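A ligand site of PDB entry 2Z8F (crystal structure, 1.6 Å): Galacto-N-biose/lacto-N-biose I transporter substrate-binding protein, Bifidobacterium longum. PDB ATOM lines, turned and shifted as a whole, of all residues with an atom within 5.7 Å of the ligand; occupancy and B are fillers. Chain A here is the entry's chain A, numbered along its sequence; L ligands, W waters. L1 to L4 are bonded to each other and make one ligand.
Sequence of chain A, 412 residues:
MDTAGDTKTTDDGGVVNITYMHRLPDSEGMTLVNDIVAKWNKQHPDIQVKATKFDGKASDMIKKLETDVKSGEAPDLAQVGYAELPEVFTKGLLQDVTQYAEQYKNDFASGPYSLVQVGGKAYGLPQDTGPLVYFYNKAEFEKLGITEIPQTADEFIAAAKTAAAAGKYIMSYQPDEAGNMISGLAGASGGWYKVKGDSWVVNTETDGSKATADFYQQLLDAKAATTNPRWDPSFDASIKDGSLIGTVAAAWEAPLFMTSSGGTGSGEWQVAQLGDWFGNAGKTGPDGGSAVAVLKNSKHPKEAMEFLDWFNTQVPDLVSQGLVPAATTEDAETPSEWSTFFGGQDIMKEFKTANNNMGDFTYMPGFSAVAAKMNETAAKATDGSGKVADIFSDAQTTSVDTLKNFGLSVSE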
ATOM      1  N   ARG A  23     -22.785  27.039 -32.273  1.00  0.00           N
ATOM      2  CA  ARG A  23     -22.346  25.666 -32.460  1.00  0.00           C
ATOM      3  C   ARG A  23     -22.899  24.743 -31.352  1.00  0.00           C
ATOM      4  O   ARG A  23     -22.219  23.844 -30.852  1.00  0.00           O
ATOM      5  CB  ARG A  23     -20.839  25.563 -32.676  1.00  0.00           C
ATOM      6  CG  ARG A  23     -19.988  26.330 -31.643  1.00  0.00           C
ATOM      7  CD  ARG A  23     -18.494  26.123 -31.950  1.00  0.00           C
ATOM      8  NE  ARG A  23     -17.595  26.888 -31.081  1.00  0.00           N
ATOM      9  CZ  ARG A  23     -17.080  26.437 -29.928  1.00  0.00           C
ATOM     10  NH1 ARG A  23     -17.423  25.255 -29.438  1.00  0.00           N
ATOM     11  NH2 ARG A  23     -16.210  27.229 -29.268  1.00  0.00           N
ATOM     12  N   LEU A  24     -24.181  24.946 -31.015  1.00  0.00           N
ATOM     13  CA  LEU A  24     -24.857  24.040 -30.115  1.00  0.00           C
ATOM     14  C   LEU A  24     -25.256  22.770 -30.866  1.00  0.00           C
ATOM     15  O   LEU A  24     -25.471  22.835 -32.092  1.00  0.00           O
ATOM     16  CB  LEU A  24     -26.076  24.726 -29.460  1.00  0.00           C
ATOM     17  CG  LEU A  24     -25.696  25.980 -28.632  1.00  0.00           C
ATOM     18  CD1 LEU A  24     -26.943  26.636 -28.036  1.00  0.00           C
ATOM     19  CD2 LEU A  24     -24.668  25.702 -27.536  1.00  0.00           C
ATOM     20  N   PRO A  25     -25.337  21.637 -30.151  1.00  0.00           N
ATOM     21  CA  PRO A  25     -25.473  20.341 -30.836  1.00  0.00           C
ATOM     22  C   PRO A  25     -26.777  20.130 -31.608  1.00  0.00           C
ATOM     23  O   PRO A  25     -26.746  19.517 -32.674  1.00  0.00           O
ATOM     24  CB  PRO A  25     -25.306  19.308 -29.710  1.00  0.00           C
ATOM     25  CG  PRO A  25     -25.585  20.049 -28.423  1.00  0.00           C
ATOM     26  CD  PRO A  25     -25.206  21.483 -28.686  1.00  0.00           C
ATOM     27  N   LYS A  57     -16.477  21.669 -37.912  1.00  0.00           N
ATOM     28  CA  LYS A  57     -15.983  21.250 -36.599  1.00  0.00           C
ATOM     29  C   LYS A  57     -15.715  22.489 -35.758  1.00  0.00           C
ATOM     30  O   LYS A  57     -15.441  23.552 -36.290  1.00  0.00           O
ATOM     31  CB  LYS A  57     -14.738  20.389 -36.727  1.00  0.00           C
ATOM     32  CG  LYS A  57     -13.495  21.104 -37.186  1.00  0.00           C
ATOM     33  CD  LYS A  57     -12.294  20.145 -37.232  1.00  0.00           C
ATOM     34  CE  LYS A  57     -11.785  19.956 -38.654  1.00  0.00           C
ATOM     35  NZ  LYS A  57     -10.803  21.053 -38.988  1.00  0.00           N
ATOM     36  N   ALA A  58     -15.789  22.334 -34.434  1.00  0.00           N
ATOM     37  CA  ALA A  58     -15.838  23.493 -33.531  1.00  0.00           C
ATOM     38  C   ALA A  58     -14.682  24.480 -33.742  1.00  0.00           C
ATOM     39  O   ALA A  58     -14.908  25.693 -33.806  1.00  0.00           O
ATOM     40  CB  ALA A  58     -15.892  23.040 -32.088  1.00  0.00           C
ATOM     41  N   SER A  59     -13.449  23.971 -33.890  1.00  0.00           N
ATOM     42  CA  SER A  59     -12.263  24.847 -33.987  1.00  0.00           C
ATOM     43  C   SER A  59     -12.200  25.677 -35.276  1.00  0.00           C
ATOM     44  O   SER A  59     -11.404  26.611 -35.406  1.00  0.00           O
ATOM     45  CB  SER A  59     -10.955  24.046 -33.833  1.00  0.00           C
ATOM     46  OG  SER A  59     -10.774  23.131 -34.920  1.00  0.00           O
ATOM     47  N   LYS A  63     -12.365  30.717 -37.214  1.00  0.00           N
ATOM     48  CA  LYS A  63     -11.700  30.930 -38.495  1.00  0.00           C
ATOM     49  C   LYS A  63     -12.691  31.443 -39.544  1.00  0.00           C
ATOM     50  O   LYS A  63     -12.383  32.401 -40.270  1.00  0.00           O
ATOM     51  CB  LYS A  63     -11.047  29.628 -38.970  1.00  0.00           C
ATOM     52  CG  LYS A  63      -9.981  29.095 -38.010  1.00  0.00           C
ATOM     53  CD  LYS A  63      -9.411  27.759 -38.497  1.00  0.00           C
ATOM     54  CE  LYS A  63      -8.142  27.385 -37.748  1.00  0.00           C
ATOM     55  NZ  LYS A  63      -8.426  26.968 -36.333  1.00  0.00           N
ATOM     56  N   GLN A  79     -21.340  32.449 -31.269  1.00  0.00           N
ATOM     57  CA  GLN A  79     -20.794  31.726 -30.110  1.00  0.00           C
ATOM     58  C   GLN A  79     -19.266  31.838 -30.114  1.00  0.00           C
ATOM     59  O   GLN A  79     -18.641  31.579 -31.135  1.00  0.00           O
ATOM     60  CB  GLN A  79     -21.205  30.258 -30.145  1.00  0.00           C
ATOM     61  CG  GLN A  79     -20.669  29.460 -28.956  1.00  0.00           C
ATOM     62  CD  GLN A  79     -21.182  28.048 -28.921  1.00  0.00           C
ATOM     63  OE1 GLN A  79     -22.190  27.728 -29.561  1.00  0.00           O
ATOM     64  NE2 GLN A  79     -20.506  27.204 -28.157  1.00  0.00           N
ATOM     65  N   GLU A  84     -11.549  31.430 -26.406  1.00  0.00           N
ATOM     66  CA  GLU A  84     -11.388  32.017 -27.726  1.00  0.00           C
ATOM     67  C   GLU A  84     -11.524  33.532 -27.734  1.00  0.00           C
ATOM     68  O   GLU A  84     -11.116  34.180 -28.692  1.00  0.00           O
ATOM     69  CB  GLU A  84     -12.459  31.462 -28.667  1.00  0.00           C
ATOM     70  CG  GLU A  84     -12.296  29.980 -28.978  1.00  0.00           C
ATOM     71  CD  GLU A  84     -13.384  29.400 -29.899  1.00  0.00           C
ATOM     72  OE1 GLU A  84     -14.574  29.785 -29.775  1.00  0.00           O
ATOM     73  OE2 GLU A  84     -13.030  28.524 -30.728  1.00  0.00           O
ATOM     74  N   GLN A 127     -22.794  32.386 -21.687  1.00  0.00           N
ATOM     75  CA  GLN A 127     -23.884  31.443 -21.981  1.00  0.00           C
ATOM     76  C   GLN A 127     -23.856  30.207 -21.094  1.00  0.00           C
ATOM     77  O   GLN A 127     -24.892  29.798 -20.557  1.00  0.00           O
ATOM     78  CB  GLN A 127     -23.906  31.078 -23.482  1.00  0.00           C
ATOM     79  CG  GLN A 127     -25.088  30.182 -23.832  1.00  0.00           C
ATOM     80  CD  GLN A 127     -25.199  29.965 -25.337  1.00  0.00           C
ATOM     81  OE1 GLN A 127     -24.483  29.108 -25.897  1.00  0.00           O
ATOM     82  NE2 GLN A 127     -26.050  30.760 -26.003  1.00  0.00           N
ATOM     83  N   ASP A 128     -22.666  29.601 -20.930  1.00  0.00           N
ATOM     84  CA  ASP A 128     -22.575  28.333 -20.169  1.00  0.00           C
ATOM     85  C   ASP A 128     -21.192  28.186 -19.527  1.00  0.00           C
ATOM     86  O   ASP A 128     -20.274  28.954 -19.838  1.00  0.00           O
ATOM     87  CB  ASP A 128     -22.859  27.117 -21.068  1.00  0.00           C
ATOM     88  CG  ASP A 128     -21.805  26.934 -22.158  1.00  0.00           C
ATOM     89  OD1 ASP A 128     -21.483  27.912 -22.887  1.00  0.00           O
ATOM     90  OD2 ASP A 128     -21.295  25.800 -22.259  1.00  0.00           O
ATOM     91  N   ASP A 176      -7.489  14.172 -29.022  1.00  0.00           N
ATOM     92  CA  ASP A 176      -8.154  15.260 -29.749  1.00  0.00           C
ATOM     93  C   ASP A 176      -8.829  16.308 -28.826  1.00  0.00           C
ATOM     94  O   ASP A 176      -9.444  17.254 -29.308  1.00  0.00           O
ATOM     95  CB  ASP A 176      -9.197  14.727 -30.750  1.00  0.00           C
ATOM     96  CG  ASP A 176     -10.281  13.862 -30.099  1.00  0.00           C
ATOM     97  OD1 ASP A 176     -10.101  13.366 -28.969  1.00  0.00           O
ATOM     98  OD2 ASP A 176     -11.349  13.639 -30.732  1.00  0.00           O
ATOM     99  N   GLU A 177      -8.672  16.115 -27.511  1.00  0.00           N
ATOM    100  CA  GLU A 177      -9.225  17.039 -26.514  1.00  0.00           C
ATOM    101  C   GLU A 177      -8.149  17.471 -25.562  1.00  0.00           C
ATOM    102  O   GLU A 177      -8.456  18.105 -24.540  1.00  0.00           O
ATOM    103  CB  GLU A 177     -10.398  16.412 -25.750  1.00  0.00           C
ATOM    104  CG  GLU A 177     -11.692  16.392 -26.613  1.00  0.00           C
ATOM    105  CD  GLU A 177     -12.257  17.810 -26.837  1.00  0.00           C
ATOM    106  OE1 GLU A 177     -11.962  18.725 -26.020  1.00  0.00           O
ATOM    107  OE2 GLU A 177     -12.995  18.015 -27.822  1.00  0.00           O
ATOM    108  N   ASN A 180      -8.176  21.196 -24.502  1.00  0.00           N
ATOM    109  CA  ASN A 180      -9.361  21.670 -23.752  1.00  0.00           C
ATOM    110  C   ASN A 180      -9.508  20.949 -22.422  1.00  0.00           C
ATOM    111  O   ASN A 180      -9.642  21.583 -21.361  1.00  0.00           O
ATOM    112  CB  ASN A 180     -10.650  21.498 -24.594  1.00  0.00           C
ATOM    113  CG  ASN A 180     -10.496  22.047 -25.996  1.00  0.00           C
ATOM    114  OD1 ASN A 180     -10.011  23.156 -26.185  1.00  0.00           O
ATOM    115  ND2 ASN A 180     -10.906  21.251 -26.999  1.00  0.00           N
ATOM    116  N   TRP A 231     -14.056  12.194 -30.417  1.00  0.00           N
ATOM    117  CA  TRP A 231     -15.074  12.492 -31.418  1.00  0.00           C
ATOM    118  C   TRP A 231     -15.110  11.463 -32.541  1.00  0.00           C
ATOM    119  O   TRP A 231     -15.892  11.618 -33.484  1.00  0.00           O
ATOM    120  CB  TRP A 231     -14.953  13.958 -31.886  1.00  0.00           C
ATOM    121  CG  TRP A 231     -15.006  14.862 -30.668  1.00  0.00           C
ATOM    122  CD1 TRP A 231     -13.963  15.552 -30.119  1.00  0.00           C
ATOM    123  CD2 TRP A 231     -16.138  15.090 -29.799  1.00  0.00           C
ATOM    124  NE1 TRP A 231     -14.369  16.199 -28.966  1.00  0.00           N
ATOM    125  CE2 TRP A 231     -15.705  15.941 -28.754  1.00  0.00           C
ATOM    126  CE3 TRP A 231     -17.472  14.653 -29.811  1.00  0.00           C
ATOM    127  CZ2 TRP A 231     -16.556  16.366 -27.719  1.00  0.00           C
ATOM    128  CZ3 TRP A 231     -18.328  15.085 -28.788  1.00  0.00           C
ATOM    129  CH2 TRP A 231     -17.861  15.929 -27.762  1.00  0.00           C
ATOM    130  N   TRP A 252     -20.978  19.579 -19.965  1.00  0.00           N
ATOM    131  CA  TRP A 252     -21.874  19.730 -21.153  1.00  0.00           C
ATOM    132  C   TRP A 252     -21.902  18.461 -22.010  1.00  0.00           C
ATOM    133  O   TRP A 252     -22.733  18.356 -22.949  1.00  0.00           O
ATOM    134  CB  TRP A 252     -21.571  20.987 -21.994  1.00  0.00           C
ATOM    135  CG  TRP A 252     -20.101  21.203 -22.264  1.00  0.00           C
ATOM    136  CD1 TRP A 252     -19.278  22.096 -21.619  1.00  0.00           C
ATOM    137  CD2 TRP A 252     -19.276  20.503 -23.207  1.00  0.00           C
ATOM    138  NE1 TRP A 252     -17.988  21.992 -22.101  1.00  0.00           N
ATOM    139  CE2 TRP A 252     -17.958  21.024 -23.065  1.00  0.00           C
ATOM    140  CE3 TRP A 252     -19.520  19.465 -24.138  1.00  0.00           C
ATOM    141  CZ2 TRP A 252     -16.883  20.552 -23.846  1.00  0.00           C
ATOM    142  CZ3 TRP A 252     -18.439  19.006 -24.914  1.00  0.00           C
ATOM    143  CH2 TRP A 252     -17.139  19.549 -24.769  1.00  0.00           C
ATOM    144  N   LEU A 256     -24.694  14.291 -24.817  1.00  0.00           N
ATOM    145  CA  LEU A 256     -23.872  13.754 -25.907  1.00  0.00           C
ATOM    146  C   LEU A 256     -23.415  12.331 -25.604  1.00  0.00           C
ATOM    147  O   LEU A 256     -23.497  11.422 -26.456  1.00  0.00           O
ATOM    148  CB  LEU A 256     -22.662  14.669 -26.141  1.00  0.00           C
ATOM    149  CG  LEU A 256     -22.952  16.173 -26.319  1.00  0.00           C
ATOM    150  CD1 LEU A 256     -21.625  16.906 -26.591  1.00  0.00           C
ATOM    151  CD2 LEU A 256     -23.969  16.463 -27.439  1.00  0.00           C
ATOM    152  N   ASP A 287     -13.309  23.212 -19.155  1.00  0.00           N
ATOM    153  CA  ASP A 287     -13.089  22.597 -20.446  1.00  0.00           C
ATOM    154  C   ASP A 287     -14.188  23.190 -21.320  1.00  0.00           C
ATOM    155  O   ASP A 287     -15.353  22.888 -21.139  1.00  0.00           O
ATOM    156  CB  ASP A 287     -13.241  21.077 -20.307  1.00  0.00           C
ATOM    157  CG  ASP A 287     -13.236  20.336 -21.669  1.00  0.00           C
ATOM    158  OD1 ASP A 287     -13.292  20.982 -22.753  1.00  0.00           O
ATOM    159  OD2 ASP A 287     -13.127  19.076 -21.591  1.00  0.00           O
ATOM    160  N   GLY A 288     -13.835  24.085 -22.236  1.00  0.00           N
ATOM    161  CA  GLY A 288     -14.869  24.837 -22.945  1.00  0.00           C
ATOM    162  C   GLY A 288     -15.712  25.753 -22.047  1.00  0.00           C
ATOM    163  O   GLY A 288     -15.237  26.281 -21.023  1.00  0.00           O
ATOM    164  N   GLY A 289     -16.969  25.927 -22.410  1.00  0.00           N
ATOM    165  CA  GLY A 289     -17.773  27.014 -21.859  1.00  0.00           C
ATOM    166  C   GLY A 289     -17.667  28.199 -22.800  1.00  0.00           C
ATOM    167  O   GLY A 289     -16.559  28.567 -23.296  1.00  0.00           O
ATOM    168  N   SER A 290     -18.821  28.800 -23.107  1.00  0.00           N
ATOM    169  CA  SER A 290     -18.869  29.835 -24.124  1.00  0.00           C
ATOM    170  C   SER A 290     -19.685  31.071 -23.795  1.00  0.00           C
ATOM    171  O   SER A 290     -20.624  31.024 -22.982  1.00  0.00           O
ATOM    172  CB  SER A 290     -19.434  29.236 -25.435  1.00  0.00           C
ATOM    173  OG  SER A 290     -18.804  28.009 -25.811  1.00  0.00           O
ATOM    174  N   GLN A 321     -29.787  21.253 -24.291  1.00  0.00           N
ATOM    175  CA  GLN A 321     -28.615  21.184 -25.187  1.00  0.00           C
ATOM    176  C   GLN A 321     -27.352  20.685 -24.468  1.00  0.00           C
ATOM    177  O   GLN A 321     -26.295  20.541 -25.086  1.00  0.00           O
ATOM    178  CB  GLN A 321     -28.347  22.575 -25.782  1.00  0.00           C
ATOM    179  CG  GLN A 321     -29.416  23.084 -26.782  1.00  0.00           C
ATOM    180  CD  GLN A 321     -29.269  22.542 -28.209  1.00  0.00           C
ATOM    181  OE1 GLN A 321     -28.194  22.099 -28.646  1.00  0.00           O
ATOM    182  NE2 GLN A 321     -30.383  22.643 -28.978  1.00  0.00           N
ATOM    183  N   LEU A 323     -26.165  22.316 -21.775  1.00  0.00           N
ATOM    184  CA  LEU A 323     -25.475  23.463 -21.166  1.00  0.00           C
ATOM    185  C   LEU A 323     -25.692  23.541 -19.681  1.00  0.00           C
ATOM    186  O   LEU A 323     -26.766  23.213 -19.158  1.00  0.00           O
ATOM    187  CB  LEU A 323     -25.915  24.787 -21.802  1.00  0.00           C
ATOM    188  CG  LEU A 323     -25.763  24.825 -23.320  1.00  0.00           C
ATOM    189  CD1 LEU A 323     -26.073  26.211 -23.825  1.00  0.00           C
ATOM    190  CD2 LEU A 323     -24.393  24.309 -23.805  1.00  0.00           C
ATOM    191  N   PHE A 367      -4.610  31.112 -28.027  1.00  0.00           N
ATOM    192  CA  PHE A 367      -4.607  29.801 -27.369  1.00  0.00           C
ATOM    193  C   PHE A 367      -5.005  28.670 -28.335  1.00  0.00           C
ATOM    194  O   PHE A 367      -4.660  27.515 -28.119  1.00  0.00           O
ATOM    195  CB  PHE A 367      -5.533  29.800 -26.129  1.00  0.00           C
ATOM    196  CG  PHE A 367      -5.472  28.525 -25.359  1.00  0.00           C
ATOM    197  CD1 PHE A 367      -4.382  28.241 -24.505  1.00  0.00           C
ATOM    198  CD2 PHE A 367      -6.472  27.563 -25.483  1.00  0.00           C
ATOM    199  CE1 PHE A 367      -4.310  27.038 -23.802  1.00  0.00           C
ATOM    200  CE2 PHE A 367      -6.414  26.360 -24.784  1.00  0.00           C
ATOM    201  CZ  PHE A 367      -5.332  26.096 -23.931  1.00  0.00           C
ATOM    202  N   SER A 368      -5.685  29.022 -29.415  1.00  0.00           N
ATOM    203  CA  SER A 368      -6.052  27.995 -30.383  1.00  0.00           C
ATOM    204  C   SER A 368      -4.838  27.237 -30.939  1.00  0.00           C
ATOM    205  O   SER A 368      -4.917  26.015 -31.172  1.00  0.00           O
ATOM    206  CB  SER A 368      -6.855  28.627 -31.513  1.00  0.00           C
ATOM    207  OG  SER A 368      -6.038  29.486 -32.289  1.00  0.00           O
ATOM    208  N   ALA A 369      -3.732  27.954 -31.143  1.00  0.00           N
ATOM    209  CA  ALA A 369      -2.480  27.344 -31.599  1.00  0.00           C
ATOM    210  C   ALA A 369      -1.868  26.467 -30.518  1.00  0.00           C
ATOM    211  O   ALA A 369      -1.240  25.462 -30.829  1.00  0.00           O
ATOM    212  CB  ALA A 369      -1.482  28.440 -32.028  1.00  0.00           C
ATOM    213  N   ALA A 371      -3.635  24.889 -28.124  1.00  0.00           N
ATOM    214  CA  ALA A 371      -4.476  23.711 -28.095  1.00  0.00           C
ATOM    215  C   ALA A 371      -4.176  22.765 -29.269  1.00  0.00           C
ATOM    216  O   ALA A 371      -4.118  21.540 -29.086  1.00  0.00           O
ATOM    217  CB  ALA A 371      -5.935  24.140 -28.074  1.00  0.00           C
ATOM    218  N   ALA A 372      -3.948  23.345 -30.445  1.00  0.00           N
ATOM    219  CA  ALA A 372      -3.590  22.561 -31.635  1.00  0.00           C
ATOM    220  C   ALA A 372      -2.303  21.758 -31.394  1.00  0.00           C
ATOM    221  O   ALA A 372      -2.258  20.545 -31.657  1.00  0.00           O
ATOM    222  CB  ALA A 372      -3.447  23.476 -32.853  1.00  0.00           C
ATOM    223  N   ASN A 375      -2.795  18.893 -28.817  1.00  0.00           N
ATOM    224  CA  ASN A 375      -3.427  17.727 -29.419  1.00  0.00           C
ATOM    225  C   ASN A 375      -2.449  16.898 -30.270  1.00  0.00           C
ATOM    226  O   ASN A 375      -2.465  15.679 -30.201  1.00  0.00           O
ATOM    227  CB  ASN A 375      -4.577  18.178 -30.314  1.00  0.00           C
ATOM    228  CG  ASN A 375      -5.833  18.582 -29.522  1.00  0.00           C
ATOM    229  OD1 ASN A 375      -5.812  18.754 -28.288  1.00  0.00           O
ATOM    230  ND2 ASN A 375      -6.949  18.695 -30.257  1.00  0.00           N
HETATM  231  C1  LIG L   1      -7.248  20.196 -34.530  1.00  0.00           C
HETATM  232  C2  LIG L   1      -8.642  20.290 -33.919  1.00  0.00           C
HETATM  233  C3  LIG L   1      -8.634  21.012 -32.547  1.00  0.00           C
HETATM  234  C4  LIG L   1      -7.816  22.310 -32.661  1.00  0.00           C
HETATM  235  C5  LIG L   1      -7.661  23.119 -31.371  1.00  0.00           C
HETATM  236  C6  LIG L   1      -6.568  21.557 -34.518  1.00  0.00           C
HETATM  237  O1  LIG L   1      -5.260  21.363 -35.019  1.00  0.00           O
HETATM  238  O2  LIG L   1      -7.317  19.736 -35.874  1.00  0.00           O
HETATM  239  O3  LIG L   1      -9.130  18.976 -33.809  1.00  0.00           O
HETATM  240  O4  LIG L   1      -9.966  21.358 -32.164  1.00  0.00           O
HETATM  241  O5  LIG L   1      -6.520  22.046 -33.181  1.00  0.00           O
HETATM  242  O6  LIG L   1      -7.318  24.450 -31.725  1.00  0.00           O
HETATM  243  C1  LG2 L   2     -10.673  20.372 -31.415  1.00  0.00           C
HETATM  244  C2  LG2 L   2     -11.827  21.154 -30.782  1.00  0.00           C
HETATM  245  C3  LG2 L   2     -12.921  20.256 -30.199  1.00  0.00           C
HETATM  246  C4  LG2 L   2     -13.338  19.182 -31.219  1.00  0.00           C
HETATM  247  C5  LG2 L   2     -12.094  18.458 -31.732  1.00  0.00           C
HETATM  248  C6  LG2 L   2     -12.423  17.443 -32.825  1.00  0.00           C
HETATM  249  O1  LG2 L   2     -11.281  21.961 -29.769  1.00  0.00           O
HETATM  250  O2  LG2 L   2     -13.948  21.186 -29.849  1.00  0.00           O
HETATM  251  O3  LG2 L   2     -13.943  19.864 -32.280  1.00  0.00           O
HETATM  252  O4  LG2 L   2     -11.198  19.389 -32.288  1.00  0.00           O
HETATM  253  O5  LG2 L   2     -11.191  16.848 -33.237  1.00  0.00           O
HETATM  254  C1  LG3 L   3     -15.061  20.663 -29.118  1.00  0.00           C
HETATM  255  C2  LG3 L   3     -15.727  21.859 -28.419  1.00  0.00           C
HETATM  256  C3  LG3 L   3     -17.108  21.553 -27.810  1.00  0.00           C
HETATM  257  C4  LG3 L   3     -17.968  20.768 -28.832  1.00  0.00           C
HETATM  258  C5  LG3 L   3     -17.160  19.558 -29.311  1.00  0.00           C
HETATM  259  C6  LG3 L   3     -17.990  18.635 -30.210  1.00  0.00           C
HETATM  260  C7  LG3 L   3     -14.443  23.616 -27.396  1.00  0.00           C
HETATM  261  C8  LG3 L   3     -13.515  24.010 -26.279  1.00  0.00           C
HETATM  262  N1  LG3 L   3     -14.800  22.353 -27.382  1.00  0.00           N
HETATM  263  O1  LG3 L   3     -17.577  22.846 -27.482  1.00  0.00           O
HETATM  264  O2  LG3 L   3     -19.129  20.302 -28.188  1.00  0.00           O
HETATM  265  O3  LG3 L   3     -16.009  20.047 -29.982  1.00  0.00           O
HETATM  266  O4  LG3 L   3     -18.293  19.314 -31.395  1.00  0.00           O
HETATM  267  O5  LG3 L   3     -14.816  24.473 -28.205  1.00  0.00           O
HETATM  268  C1  LG4 L   4     -18.529  22.895 -26.412  1.00  0.00           C
HETATM  269  C2  LG4 L   4     -18.490  24.312 -25.840  1.00  0.00           C
HETATM  270  C3  LG4 L   4     -19.588  24.450 -24.793  1.00  0.00           C
HETATM  271  C4  LG4 L   4     -20.952  24.062 -25.399  1.00  0.00           C
HETATM  272  C5  LG4 L   4     -20.892  22.649 -25.984  1.00  0.00           C
HETATM  273  C6  LG4 L   4     -22.173  22.252 -26.711  1.00  0.00           C
HETATM  274  O1  LG4 L   4     -17.231  24.511 -25.207  1.00  0.00           O
HETATM  275  O2  LG4 L   4     -19.578  25.776 -24.344  1.00  0.00           O
HETATM  276  O3  LG4 L   4     -21.249  25.035 -26.364  1.00  0.00           O
HETATM  277  O4  LG4 L   4     -19.831  22.576 -26.932  1.00  0.00           O
HETATM  278  O5  LG4 L   4     -22.160  20.850 -26.943  1.00  0.00           O
HETATM  279  O   HOH W   1     -12.947  26.073 -29.209  1.00  0.00           O
HETATM  280  O   HOH W   2      -5.087  19.231 -37.637  1.00  0.00           O
HETATM  281  O   HOH W   3     -21.565  19.619 -29.328  1.00  0.00           O
HETATM  282  O   HOH W   4      -3.567  19.556 -33.711  1.00  0.00           O
HETATM  283  O   HOH W   5      -4.727  23.686 -36.451  1.00  0.00           O
HETATM  284  O   HOH W   6     -13.960  20.543 -25.414  1.00  0.00           O
HETATM  285  O   HOH W   7     -19.400  21.741 -32.263  1.00  0.00           O
HETATM  286  O   HOH W   8     -12.632  21.209 -34.222  1.00  0.00           O
HETATM  287  O   HOH W   9     -16.569  19.833 -33.365  1.00  0.00           O
HETATM  288  O   HOH W  10     -22.308  27.432 -25.293  1.00  0.00           O
HETATM  289  O   HOH W  11     -11.086  24.574 -30.488  1.00  0.00           O
HETATM  290  O   HOH W  12     -11.220  14.137 -33.355  1.00  0.00           O
HETATM  291  O   HOH W  13      -7.324  25.790 -34.095  1.00  0.00           O
HETATM  292  O   HOH W  14     -23.635  19.805 -25.154  1.00  0.00           O
HETATM  293  O   HOH W  15     -16.161  26.754 -26.311  1.00  0.00           O
HETATM  294  O   HOH W  16      -8.275  21.376 -38.142  1.00  0.00           O
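An oxygen (O2) of LG4 L4 is in hydrogen-bond range of the side-chain carboxylate (OD2) of Asp 128 (2.7 Å). The side-chain amide nitrogen (NE2) of Gln 79 is in hydrogen-bond range of an oxygen (O3) of LG4 L4 (2.9 Å). The side-chain hydroxyl (OG) of Ser 59 lies close to an oxygen (O4) of LIG L1 (3.4 Å). The backbone carbonyl oxygen (O) of Ser 368 is in hydrogen-bond range of an oxygen (O6) of LIG L1 (2.9 Å). ND2 of Asn 180 is in hydrogen-bond range of O1 of LG2 L2, 2.9 Å away. An oxygen (O2) of LG4 L4 is in hydrogen-bond range of the backbone NH (N) of Ser 290 (3.4 Å). An oxygen (O1) of LG4 L4 lies within hydrogen-bond range of the backbone NH (N) of Gly 289 (3.1 Å). The guanidinium group of Arg 23 lies within hydrogen-bond range of an oxygen (O5) of LG3 L3 (3.0 Å). An oxygen (O2) of LG4 L4 is in hydrogen-bond range of the side-chain hydroxyl of Ser 290, 2.8 Å away.
The side-chain amide oxygen (OE1) of Gln 79 lies within hydrogen-bond range of the backbone NH (N) of Arg 23 (2.9 Å). O of Ser 59 is in hydrogen-bond range of NZ of Lys 63, 3.1 Å away. The backbone NH (N) of Ser 290 sits at hydrogen-bond distance from the side-chain carboxylate (OD1) of Asp 128, 2.8 Å away. The backbone NH (N) of Trp 231 sits at hydrogen-bond distance from the side-chain carboxylate (OD2) of Asp 176 (3.1 Å). The backbone NH of Gln 127 lies within hydrogen-bond range of the backbone carbonyl oxygen of Ser 290 (2.9 Å). The side-chain amide oxygen (OD1) of Asn 375 sits close to the backbone carbonyl oxygen (O) of Ala 371 (3.4 Å). NH2 of Arg 23 lies within salt-bridge range of OE1 of Glu 84 (3.1 Å). The backbone carbonyl oxygen (O) of Asp 287 sits at hydrogen-bond distance from the indole nitrogen (NE1) of Trp 252 (2.9 Å).
Merely in contact with the ligand: Glu 177, Gly 288, Ala 372, Ala 58, Pro 25, Trp 252, Trp 231, Asn 375, Leu 24, Asp 176, Leu 323, Ala 371 and Leu 256. Hydrophobic or aromatic side chains that line the ligand: Leu 24, Pro 25, Ala 58, Trp 231, Trp 252, Leu 256, Leu 323, Ala 371 and Ala 372. Within 4 Å of the ligand: Arg 23, Leu 24, Pro 25, Ala 58, Ser 59, Gln 79, Asp 128, Asp 176, Glu 177, Asn 180, Trp 231, Trp 252, Leu 256, Gly 288, Gly 289, Ser 290, Leu 323, Ser 368, Ala 371, Ala 372 and Asn 375. The nearest printed residue that does not touch the ligand is Gln 321 (4.5 Å).
Water W8 lies within hydrogen-bond range of O3 of LG2 L2, OG of Ser 59 and N of Ala 58. Water W15 lies within hydrogen-bond range of an oxygen (O1) of LG4 L4, the side-chain hydroxyl (OG) of Ser 290 and the guanidinium group (NH2) of Arg 23. Water W4 bridges O of Ala 372 (2.6 Å) and O1 of LIG L1 (2.8 Å). Water W6 lies within hydrogen-bond range of the side-chain carboxylate of Glu 177 (2.8 Å), the side-chain carboxylate of Asp 287 (2.8 Å) and a nitrogen (N1) of LG3 L3 (2.8 Å). Water W10 lies within hydrogen-bond range of the side-chain carboxylate of Asp 128 (2.6 Å), the side-chain amide oxygen of Gln 127 (2.8 Å), an oxygen (O3) of LG4 L4 (2.8 Å) and the side-chain amide nitrogen of Gln 79 (3.4 Å). Water W16 lies within hydrogen-bond range of the side-chain amino group (NZ) of Lys 57 and an oxygen (O2) of LIG L1.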
